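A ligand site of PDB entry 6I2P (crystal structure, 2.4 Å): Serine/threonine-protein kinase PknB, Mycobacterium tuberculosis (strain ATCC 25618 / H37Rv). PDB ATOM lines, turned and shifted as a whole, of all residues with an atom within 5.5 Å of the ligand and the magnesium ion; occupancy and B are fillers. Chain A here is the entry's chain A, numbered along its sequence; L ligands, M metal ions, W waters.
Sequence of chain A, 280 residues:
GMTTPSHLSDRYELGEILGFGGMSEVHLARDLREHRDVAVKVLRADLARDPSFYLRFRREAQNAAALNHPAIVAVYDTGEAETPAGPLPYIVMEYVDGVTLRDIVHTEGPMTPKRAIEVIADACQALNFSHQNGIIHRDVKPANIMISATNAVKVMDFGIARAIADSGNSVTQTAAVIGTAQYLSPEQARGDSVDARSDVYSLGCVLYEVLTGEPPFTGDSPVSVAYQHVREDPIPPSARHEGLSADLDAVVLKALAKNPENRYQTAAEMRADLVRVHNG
The magnesium ion is bound by O2 of the ligand (2.5 Å). The magnesium ion has one donor atom within binding distance. Slightly farther from the magnesium ion lies O5 of the ligand (2.6 Å).
OE2 of Glu 60 touches the magnesium ion, 3.4 Å away. OD1 of Asp 157 touches the magnesium ion, at 3.0 Å. Of the 26 residues printed, 2 come within 4 Å of the magnesium ion. The nearest printed residue that does not touch the magnesium ion is TPO 174 (4.2 Å).
Residues that only touch the ligand: Leu 18, Gly 19, Phe 20, Gly 21, Val 26, Ala 39, Glu 60, Val 73, Met 93, Tyr 95, Thr 100, Met 146 and Met 156. Hydrophobic or aromatic side chains that line the ligand: Leu 18, Val 26, Ala 39, Val 73, Met 93, Val 96, Met 146 and Met 156. The nearest printed residue that does not touch the ligand is Lys 141 (4.2 Å).
N of Val 26 is in hydrogen-bond range of O of Gly 19 (2.9 Å). The backbone NH (N) of Leu 18 is in hydrogen-bond range of the backbone carbonyl oxygen (O) of Val 26. The backbone carbonyl oxygen (O) of Ala 39 is in hydrogen-bond range of the backbone NH (N) of Met 93 (2.7 Å). The backbone NH of Met 156 is in hydrogen-bond range of the backbone carbonyl oxygen of Asn 144 (2.8 Å). OG1 of Thr 100 sits at hydrogen-bond distance from OD2 of Asp 103 (3.1 Å). OH of Tyr 95 is in hydrogen-bond range of OD1 of Asp 97.
The side-chain hydroxyl (OG) of Ser 24 is in hydrogen-bond range of an oxygen (O4) of the ligand (2.7 Å). O5 of the ligand is in salt-bridge range of NZ of Lys 41. A nitrogen (N3) of the ligand sits at hydrogen-bond distance from the backbone carbonyl oxygen (O) of Glu 94 (2.8 Å). N4 of the ligand sits at hydrogen-bond distance from N of Val 96 (3.0 Å). The backbone NH of Gly 22 sits at hydrogen-bond distance from an oxygen (O1) of the ligand, at 3.1 Å.
Water W4 bridges an oxygen (O7) of the ligand (2.7 Å) and the backbone carbonyl oxygen (O) of Ala 143 (2.7 Å). Water W1 bridges O7 of the ligand (2.7 Å) and OD1 of Asn 144 (2.7 Å).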
ATOM      1  N   LEU A  18      17.440  -9.276 -34.271  1.00  0.00           N
ATOM      2  CA  LEU A  18      17.065  -8.066 -33.525  1.00  0.00           C
ATOM      3  C   LEU A  18      18.096  -7.685 -32.466  1.00  0.00           C
ATOM      4  O   LEU A  18      18.349  -6.497 -32.230  1.00  0.00           O
ATOM      5  CB  LEU A  18      15.667  -8.247 -32.884  1.00  0.00           C
ATOM      6  CG  LEU A  18      14.492  -8.426 -33.860  1.00  0.00           C
ATOM      7  CD1 LEU A  18      13.248  -8.871 -33.130  1.00  0.00           C
ATOM      8  CD2 LEU A  18      14.218  -7.154 -34.668  1.00  0.00           C
ATOM      9  N   GLY A  19      18.711  -8.695 -31.877  1.00  0.00           N
ATOM     10  CA  GLY A  19      19.702  -8.536 -30.840  1.00  0.00           C
ATOM     11  C   GLY A  19      20.283  -9.840 -30.348  1.00  0.00           C
ATOM     12  O   GLY A  19      19.895 -10.922 -30.795  1.00  0.00           O
ATOM     13  N   PHE A  20      21.198  -9.727 -29.396  1.00  0.00           N
ATOM     14  CA  PHE A  20      21.918 -10.850 -28.825  1.00  0.00           C
ATOM     15  C   PHE A  20      21.909 -10.771 -27.325  1.00  0.00           C
ATOM     16  O   PHE A  20      22.038  -9.689 -26.742  1.00  0.00           O
ATOM     17  CB  PHE A  20      23.388 -10.863 -29.319  1.00  0.00           C
ATOM     18  CG  PHE A  20      23.571 -11.017 -30.798  1.00  0.00           C
ATOM     19  CD1 PHE A  20      23.613 -12.280 -31.392  1.00  0.00           C
ATOM     20  CD2 PHE A  20      23.727  -9.904 -31.615  1.00  0.00           C
ATOM     21  CE1 PHE A  20      23.761 -12.414 -32.770  1.00  0.00           C
ATOM     22  CE2 PHE A  20      23.883 -10.042 -32.998  1.00  0.00           C
ATOM     23  CZ  PHE A  20      23.912 -11.292 -33.559  1.00  0.00           C
ATOM     24  N   GLY A  21      21.797 -11.936 -26.696  1.00  0.00           N
ATOM     25  CA  GLY A  21      21.860 -12.078 -25.249  1.00  0.00           C
ATOM     26  C   GLY A  21      23.217 -12.619 -24.866  1.00  0.00           C
ATOM     27  O   GLY A  21      24.225 -12.234 -25.450  1.00  0.00           O
ATOM     28  N   GLY A  22      23.241 -13.528 -23.898  1.00  0.00           N
ATOM     29  CA  GLY A  22      24.478 -14.168 -23.442  1.00  0.00           C
ATOM     30  C   GLY A  22      24.908 -15.284 -24.373  1.00  0.00           C
ATOM     31  O   GLY A  22      25.994 -15.244 -24.960  1.00  0.00           O
ATOM     32  N   MET A  23      24.032 -16.291 -24.526  1.00  0.00           N
ATOM     33  CA  MET A  23      24.239 -17.470 -25.374  1.00  0.00           C
ATOM     34  C   MET A  23      23.196 -17.513 -26.487  1.00  0.00           C
ATOM     35  O   MET A  23      23.155 -18.449 -27.295  1.00  0.00           O
ATOM     36  CB  MET A  23      24.171 -18.755 -24.518  1.00  0.00           C
ATOM     37  CG  MET A  23      22.779 -19.053 -23.974  1.00  0.00           C
ATOM     38  SD  MET A  23      22.661 -20.625 -23.114  1.00  0.00           S
ATOM     39  CE  MET A  23      23.220 -20.144 -21.509  1.00  0.00           C
ATOM     40  N   SER A  24      22.340 -16.490 -26.533  1.00  0.00           N
ATOM     41  CA  SER A  24      21.230 -16.409 -27.461  1.00  0.00           C
ATOM     42  C   SER A  24      21.318 -15.309 -28.521  1.00  0.00           C
ATOM     43  O   SER A  24      22.133 -14.394 -28.423  1.00  0.00           O
ATOM     44  CB  SER A  24      19.930 -16.265 -26.689  1.00  0.00           C
ATOM     45  OG  SER A  24      19.791 -14.952 -26.182  1.00  0.00           O
ATOM     46  N   VAL A  26      18.129 -13.194 -30.952  1.00  0.00           N
ATOM     47  CA  VAL A  26      16.698 -12.992 -31.157  1.00  0.00           C
ATOM     48  C   VAL A  26      16.482 -12.602 -32.608  1.00  0.00           C
ATOM     49  O   VAL A  26      17.109 -11.663 -33.073  1.00  0.00           O
ATOM     50  CB  VAL A  26      16.068 -11.978 -30.156  1.00  0.00           C
ATOM     51  CG1 VAL A  26      14.545 -11.897 -30.329  1.00  0.00           C
ATOM     52  CG2 VAL A  26      16.407 -12.333 -28.706  1.00  0.00           C
ATOM     53  N   ALA A  39       9.013 -12.443 -32.298  1.00  0.00           N
ATOM     54  CA  ALA A  39      10.438 -12.411 -31.960  1.00  0.00           C
ATOM     55  C   ALA A  39      10.792 -13.812 -31.471  1.00  0.00           C
ATOM     56  O   ALA A  39      10.156 -14.303 -30.553  1.00  0.00           O
ATOM     57  CB  ALA A  39      10.695 -11.379 -30.870  1.00  0.00           C
ATOM     58  N   LYS A  41      13.613 -16.143 -29.807  1.00  0.00           N
ATOM     59  CA  LYS A  41      14.880 -16.239 -29.089  1.00  0.00           C
ATOM     60  C   LYS A  41      15.389 -17.653 -29.271  1.00  0.00           C
ATOM     61  O   LYS A  41      14.710 -18.629 -28.973  1.00  0.00           O
ATOM     62  CB  LYS A  41      14.730 -15.895 -27.590  1.00  0.00           C
ATOM     63  CG  LYS A  41      16.090 -15.817 -26.865  1.00  0.00           C
ATOM     64  CD  LYS A  41      15.945 -15.769 -25.346  1.00  0.00           C
ATOM     65  CE  LYS A  41      15.783 -14.360 -24.842  1.00  0.00           C
ATOM     66  NZ  LYS A  41      15.488 -14.344 -23.393  1.00  0.00           N
ATOM     67  N   GLU A  60      15.870 -23.005 -20.121  1.00  0.00           N
ATOM     68  CA  GLU A  60      15.396 -21.638 -20.331  1.00  0.00           C
ATOM     69  C   GLU A  60      14.099 -21.632 -21.145  1.00  0.00           C
ATOM     70  O   GLU A  60      13.161 -20.933 -20.747  1.00  0.00           O
ATOM     71  CB  GLU A  60      16.491 -20.815 -21.035  1.00  0.00           C
ATOM     72  CG  GLU A  60      16.400 -19.310 -20.801  1.00  0.00           C
ATOM     73  CD  GLU A  60      17.681 -18.536 -21.059  1.00  0.00           C
ATOM     74  OE1 GLU A  60      18.742 -18.928 -20.510  1.00  0.00           O
ATOM     75  OE2 GLU A  60      17.616 -17.527 -21.792  1.00  0.00           O
ATOM     76  N   VAL A  73       6.147  -8.824 -22.078  1.00  0.00           N
ATOM     77  CA  VAL A  73       6.439  -9.462 -23.362  1.00  0.00           C
ATOM     78  C   VAL A  73       5.844 -10.877 -23.279  1.00  0.00           C
ATOM     79  O   VAL A  73       6.242 -11.665 -22.415  1.00  0.00           O
ATOM     80  CB  VAL A  73       7.942  -9.476 -23.727  1.00  0.00           C
ATOM     81  CG1 VAL A  73       8.194 -10.350 -24.949  1.00  0.00           C
ATOM     82  CG2 VAL A  73       8.474  -8.069 -23.959  1.00  0.00           C
ATOM     83  N   MET A  93       8.195 -15.175 -28.863  1.00  0.00           N
ATOM     84  CA  MET A  93       7.736 -14.046 -28.067  1.00  0.00           C
ATOM     85  C   MET A  93       6.984 -13.028 -28.882  1.00  0.00           C
ATOM     86  O   MET A  93       7.065 -13.001 -30.114  1.00  0.00           O
ATOM     87  CB  MET A  93       8.944 -13.299 -27.442  1.00  0.00           C
ATOM     88  CG  MET A  93       9.750 -14.100 -26.460  1.00  0.00           C
ATOM     89  SD  MET A  93      11.316 -13.259 -26.100  1.00  0.00           S
ATOM     90  CE  MET A  93      12.158 -13.392 -27.647  1.00  0.00           C
ATOM     91  N   GLU A  94       6.322 -12.119 -28.170  1.00  0.00           N
ATOM     92  CA  GLU A  94       5.655 -10.963 -28.728  1.00  0.00           C
ATOM     93  C   GLU A  94       6.801 -10.053 -29.250  1.00  0.00           C
ATOM     94  O   GLU A  94       7.735  -9.723 -28.492  1.00  0.00           O
ATOM     95  CB  GLU A  94       4.863 -10.262 -27.616  1.00  0.00           C
ATOM     96  CG  GLU A  94       4.227  -8.944 -28.017  1.00  0.00           C
ATOM     97  CD  GLU A  94       3.767  -8.098 -26.859  1.00  0.00           C
ATOM     98  OE1 GLU A  94       3.440  -6.913 -27.097  1.00  0.00           O
ATOM     99  OE2 GLU A  94       3.717  -8.605 -25.710  1.00  0.00           O
ATOM    100  N   TYR A  95       6.747  -9.695 -30.541  1.00  0.00           N
ATOM    101  CA  TYR A  95       7.749  -8.818 -31.147  1.00  0.00           C
ATOM    102  C   TYR A  95       7.585  -7.397 -30.636  1.00  0.00           C
ATOM    103  O   TYR A  95       6.501  -6.818 -30.736  1.00  0.00           O
ATOM    104  CB  TYR A  95       7.707  -8.868 -32.699  1.00  0.00           C
ATOM    105  CG  TYR A  95       8.449  -7.740 -33.384  1.00  0.00           C
ATOM    106  CD1 TYR A  95       9.811  -7.539 -33.174  1.00  0.00           C
ATOM    107  CD2 TYR A  95       7.799  -6.884 -34.263  1.00  0.00           C
ATOM    108  CE1 TYR A  95      10.503  -6.500 -33.788  1.00  0.00           C
ATOM    109  CE2 TYR A  95       8.478  -5.838 -34.905  1.00  0.00           C
ATOM    110  CZ  TYR A  95       9.833  -5.655 -34.667  1.00  0.00           C
ATOM    111  OH  TYR A  95      10.516  -4.635 -35.278  1.00  0.00           O
ATOM    112  N   VAL A  96       8.666  -6.844 -30.078  1.00  0.00           N
ATOM    113  CA  VAL A  96       8.695  -5.473 -29.586  1.00  0.00           C
ATOM    114  C   VAL A  96       9.591  -4.651 -30.504  1.00  0.00           C
ATOM    115  O   VAL A  96      10.814  -4.856 -30.525  1.00  0.00           O
ATOM    116  CB  VAL A  96       9.117  -5.361 -28.090  1.00  0.00           C
ATOM    117  CG1 VAL A  96       9.169  -3.901 -27.649  1.00  0.00           C
ATOM    118  CG2 VAL A  96       8.169  -6.163 -27.193  1.00  0.00           C
ATOM    119  N   ASP A  97       8.986  -3.735 -31.271  1.00  0.00           N
ATOM    120  CA  ASP A  97       9.714  -2.831 -32.161  1.00  0.00           C
ATOM    121  C   ASP A  97      10.130  -1.642 -31.297  1.00  0.00           C
ATOM    122  O   ASP A  97       9.348  -0.716 -31.089  1.00  0.00           O
ATOM    123  CB  ASP A  97       8.831  -2.400 -33.349  1.00  0.00           C
ATOM    124  CG  ASP A  97       9.494  -1.412 -34.305  1.00  0.00           C
ATOM    125  OD1 ASP A  97      10.746  -1.461 -34.438  1.00  0.00           O
ATOM    126  OD2 ASP A  97       8.767  -0.605 -34.924  1.00  0.00           O
ATOM    127  N   THR A 100      15.728  -1.335 -25.310  1.00  0.00           N
ATOM    128  CA  THR A 100      15.719  -1.578 -23.861  1.00  0.00           C
ATOM    129  C   THR A 100      15.940  -0.252 -23.119  1.00  0.00           C
ATOM    130  O   THR A 100      16.366   0.734 -23.738  1.00  0.00           O
ATOM    131  CB  THR A 100      16.761  -2.648 -23.461  1.00  0.00           C
ATOM    132  OG1 THR A 100      18.078  -2.121 -23.602  1.00  0.00           O
ATOM    133  CG2 THR A 100      16.628  -3.954 -24.274  1.00  0.00           C
ATOM    134  N   ASP A 103      19.624   0.701 -23.334  1.00  0.00           N
ATOM    135  CA  ASP A 103      19.970   1.389 -24.582  1.00  0.00           C
ATOM    136  C   ASP A 103      19.668   2.884 -24.505  1.00  0.00           C
ATOM    137  O   ASP A 103      20.489   3.685 -24.964  1.00  0.00           O
ATOM    138  CB  ASP A 103      19.232   0.760 -25.777  1.00  0.00           C
ATOM    139  CG  ASP A 103      19.566  -0.691 -26.071  1.00  0.00           C
ATOM    140  OD1 ASP A 103      20.714  -1.098 -25.807  1.00  0.00           O
ATOM    141  OD2 ASP A 103      18.675  -1.407 -26.578  1.00  0.00           O
ATOM    142  N   LYS A 141      15.937  -5.146 -14.161  1.00  0.00           N
ATOM    143  CA  LYS A 141      17.065  -4.320 -14.583  1.00  0.00           C
ATOM    144  C   LYS A 141      16.692  -3.561 -15.874  1.00  0.00           C
ATOM    145  O   LYS A 141      15.752  -4.003 -16.549  1.00  0.00           O
ATOM    146  CB  LYS A 141      18.344  -5.193 -14.768  1.00  0.00           C
ATOM    147  CG  LYS A 141      18.267  -6.285 -15.820  1.00  0.00           C
ATOM    148  CD  LYS A 141      19.477  -7.192 -15.726  1.00  0.00           C
ATOM    149  CE  LYS A 141      19.470  -8.272 -16.779  1.00  0.00           C
ATOM    150  NZ  LYS A 141      20.603  -9.221 -16.617  1.00  0.00           N
ATOM    151  N   ALA A 143      17.871  -3.574 -18.868  1.00  0.00           N
ATOM    152  CA  ALA A 143      17.928  -4.459 -20.034  1.00  0.00           C
ATOM    153  C   ALA A 143      16.671  -5.340 -20.195  1.00  0.00           C
ATOM    154  O   ALA A 143      16.359  -5.761 -21.313  1.00  0.00           O
ATOM    155  CB  ALA A 143      19.162  -5.335 -19.976  1.00  0.00           C
ATOM    156  N   ASN A 144      15.936  -5.594 -19.083  1.00  0.00           N
ATOM    157  CA  ASN A 144      14.721  -6.400 -19.090  1.00  0.00           C
ATOM    158  C   ASN A 144      13.419  -5.590 -19.267  1.00  0.00           C
ATOM    159  O   ASN A 144      12.318  -6.137 -19.136  1.00  0.00           O
ATOM    160  CB  ASN A 144      14.655  -7.289 -17.845  1.00  0.00           C
ATOM    161  CG  ASN A 144      15.449  -8.552 -18.000  1.00  0.00           C
ATOM    162  OD1 ASN A 144      15.684  -9.067 -19.125  1.00  0.00           O
ATOM    163  ND2 ASN A 144      15.880  -9.095 -16.879  1.00  0.00           N
ATOM    164  N   MET A 146      11.695  -2.973 -22.122  1.00  0.00           N
ATOM    165  CA  MET A 146      11.734  -2.411 -23.460  1.00  0.00           C
ATOM    166  C   MET A 146      10.668  -1.316 -23.632  1.00  0.00           C
ATOM    167  O   MET A 146       9.622  -1.356 -22.975  1.00  0.00           O
ATOM    168  CB  MET A 146      11.547  -3.506 -24.520  1.00  0.00           C
ATOM    169  CG  MET A 146      12.772  -4.392 -24.696  1.00  0.00           C
ATOM    170  SD  MET A 146      12.644  -5.533 -26.084  1.00  0.00           S
ATOM    171  CE  MET A 146      13.004  -4.442 -27.451  1.00  0.00           C
ATOM    172  N   MET A 156      10.262  -7.959 -19.725  1.00  0.00           N
ATOM    173  CA  MET A 156      10.577  -9.324 -20.165  1.00  0.00           C
ATOM    174  C   MET A 156      11.372 -10.096 -19.120  1.00  0.00           C
ATOM    175  O   MET A 156      11.719  -9.549 -18.073  1.00  0.00           O
ATOM    176  CB  MET A 156      11.280  -9.315 -21.535  1.00  0.00           C
ATOM    177  CG  MET A 156      12.607  -8.570 -21.565  1.00  0.00           C
ATOM    178  SD  MET A 156      13.042  -8.100 -23.250  1.00  0.00           S
ATOM    179  CE  MET A 156      14.791  -7.997 -23.098  1.00  0.00           C
ATOM    180  N   ASP A 157      11.624 -11.382 -19.410  1.00  0.00           N
ATOM    181  CA  ASP A 157      12.391 -12.343 -18.605  1.00  0.00           C
ATOM    182  C   ASP A 157      11.736 -12.678 -17.267  1.00  0.00           C
ATOM    183  O   ASP A 157      12.361 -12.570 -16.207  1.00  0.00           O
ATOM    184  CB  ASP A 157      13.865 -11.892 -18.433  1.00  0.00           C
ATOM    185  CG  ASP A 157      14.815 -13.001 -18.018  1.00  0.00           C
ATOM    186  OD1 ASP A 157      14.935 -13.999 -18.773  1.00  0.00           O
ATOM    187  OD2 ASP A 157      15.440 -12.885 -16.943  1.00  0.00           O
ATOM    188  N   TPO A 174      18.578 -20.626 -13.002  1.00  0.00           N
ATOM    189  CA  TPO A 174      19.932 -20.104 -12.843  1.00  0.00           C
ATOM    190  CB  TPO A 174      20.523 -19.536 -14.148  1.00  0.00           C
ATOM    191  CG2 TPO A 174      21.239 -20.661 -14.882  1.00  0.00           C
ATOM    192  OG1 TPO A 174      19.527 -19.043 -15.055  1.00  0.00           O
ATOM    193  P   TPO A 174      19.459 -17.490 -15.194  1.00  0.00           P
ATOM    194  O1P TPO A 174      18.995 -17.261 -16.642  1.00  0.00           O
ATOM    195  O2P TPO A 174      18.381 -16.949 -14.241  1.00  0.00           O
ATOM    196  O3P TPO A 174      20.792 -16.740 -14.970  1.00  0.00           O
ATOM    197  C   TPO A 174      20.005 -19.114 -11.669  1.00  0.00           C
ATOM    198  O   TPO A 174      18.974 -18.580 -11.263  1.00  0.00           O
HETATM  199  P1  LIG L   1      20.957 -13.021 -20.475  1.00  0.00           P
HETATM  200  O1  LIG L   1      21.984 -13.992 -21.094  1.00  0.00           O
HETATM  201  O2  LIG L   1      19.928 -13.730 -19.636  1.00  0.00           O
HETATM  202  O3  LIG L   1      21.695 -11.903 -19.720  1.00  0.00           O
HETATM  203  P2  LIG L   1      19.085 -13.098 -22.880  1.00  0.00           P
HETATM  204  O4  LIG L   1      19.887 -14.223 -23.577  1.00  0.00           O
HETATM  205  O5  LIG L   1      17.912 -13.744 -22.179  1.00  0.00           O
HETATM  206  C1  LIG L   1      20.258 -12.165 -21.895  1.00  0.00           C
HETATM  207  P3  LIG L   1      17.706 -10.758 -23.968  1.00  0.00           P
HETATM  208  O6  LIG L   1      16.316 -11.185 -23.514  1.00  0.00           O
HETATM  209  O7  LIG L   1      18.319  -9.702 -23.121  1.00  0.00           O
HETATM  210  O8  LIG L   1      18.608 -12.073 -24.017  1.00  0.00           O
HETATM  211  O9  LIG L   1      17.590 -10.294 -25.524  1.00  0.00           O
HETATM  212  C2  LIG L   1      18.706  -9.774 -26.263  1.00  0.00           C
HETATM  213  C3  LIG L   1      18.238  -8.621 -27.129  1.00  0.00           C
HETATM  214  O10 LIG L   1      17.245  -9.094 -28.072  1.00  0.00           O
HETATM  215  C4  LIG L   1      17.571  -7.454 -26.398  1.00  0.00           C
HETATM  216  O11 LIG L   1      18.527  -6.543 -25.888  1.00  0.00           O
HETATM  217  C5  LIG L   1      16.664  -6.857 -27.482  1.00  0.00           C
HETATM  218  O12 LIG L   1      17.370  -5.960 -28.335  1.00  0.00           O
HETATM  219  C6  LIG L   1      16.246  -8.109 -28.262  1.00  0.00           C
HETATM  220  N1  LIG L   1      14.938  -8.655 -27.879  1.00  0.00           N
HETATM  221  C7  LIG L   1      14.694  -9.614 -26.924  1.00  0.00           C
HETATM  222  N2  LIG L   1      13.440  -9.985 -26.858  1.00  0.00           N
HETATM  223  C8  LIG L   1      12.811  -9.210 -27.819  1.00  0.00           C
HETATM  224  C9  LIG L   1      11.463  -9.128 -28.256  1.00  0.00           C
HETATM  225  N3  LIG L   1      10.455  -9.843 -27.738  1.00  0.00           N
HETATM  226  N4  LIG L   1      11.187  -8.260 -29.261  1.00  0.00           N
HETATM  227  C10 LIG L   1      12.175  -7.519 -29.771  1.00  0.00           C
HETATM  228  N5  LIG L   1      13.472  -7.505 -29.433  1.00  0.00           N
HETATM  229  C11 LIG L   1      13.732  -8.380 -28.450  1.00  0.00           C
HETATM  230 MG    MG M   1      17.688 -14.803 -19.803  1.00  0.00          MG
HETATM  231  O   HOH W   1      17.992  -9.664 -20.428  1.00  0.00           O
HETATM  232  O   HOH W   2      20.991  -9.047 -23.053  1.00  0.00           O
HETATM  233  O   HOH W   3      15.204  -5.531 -30.760  1.00  0.00           O
HETATM  234  O   HOH W   4      18.065  -7.006 -23.049  1.00  0.00           O
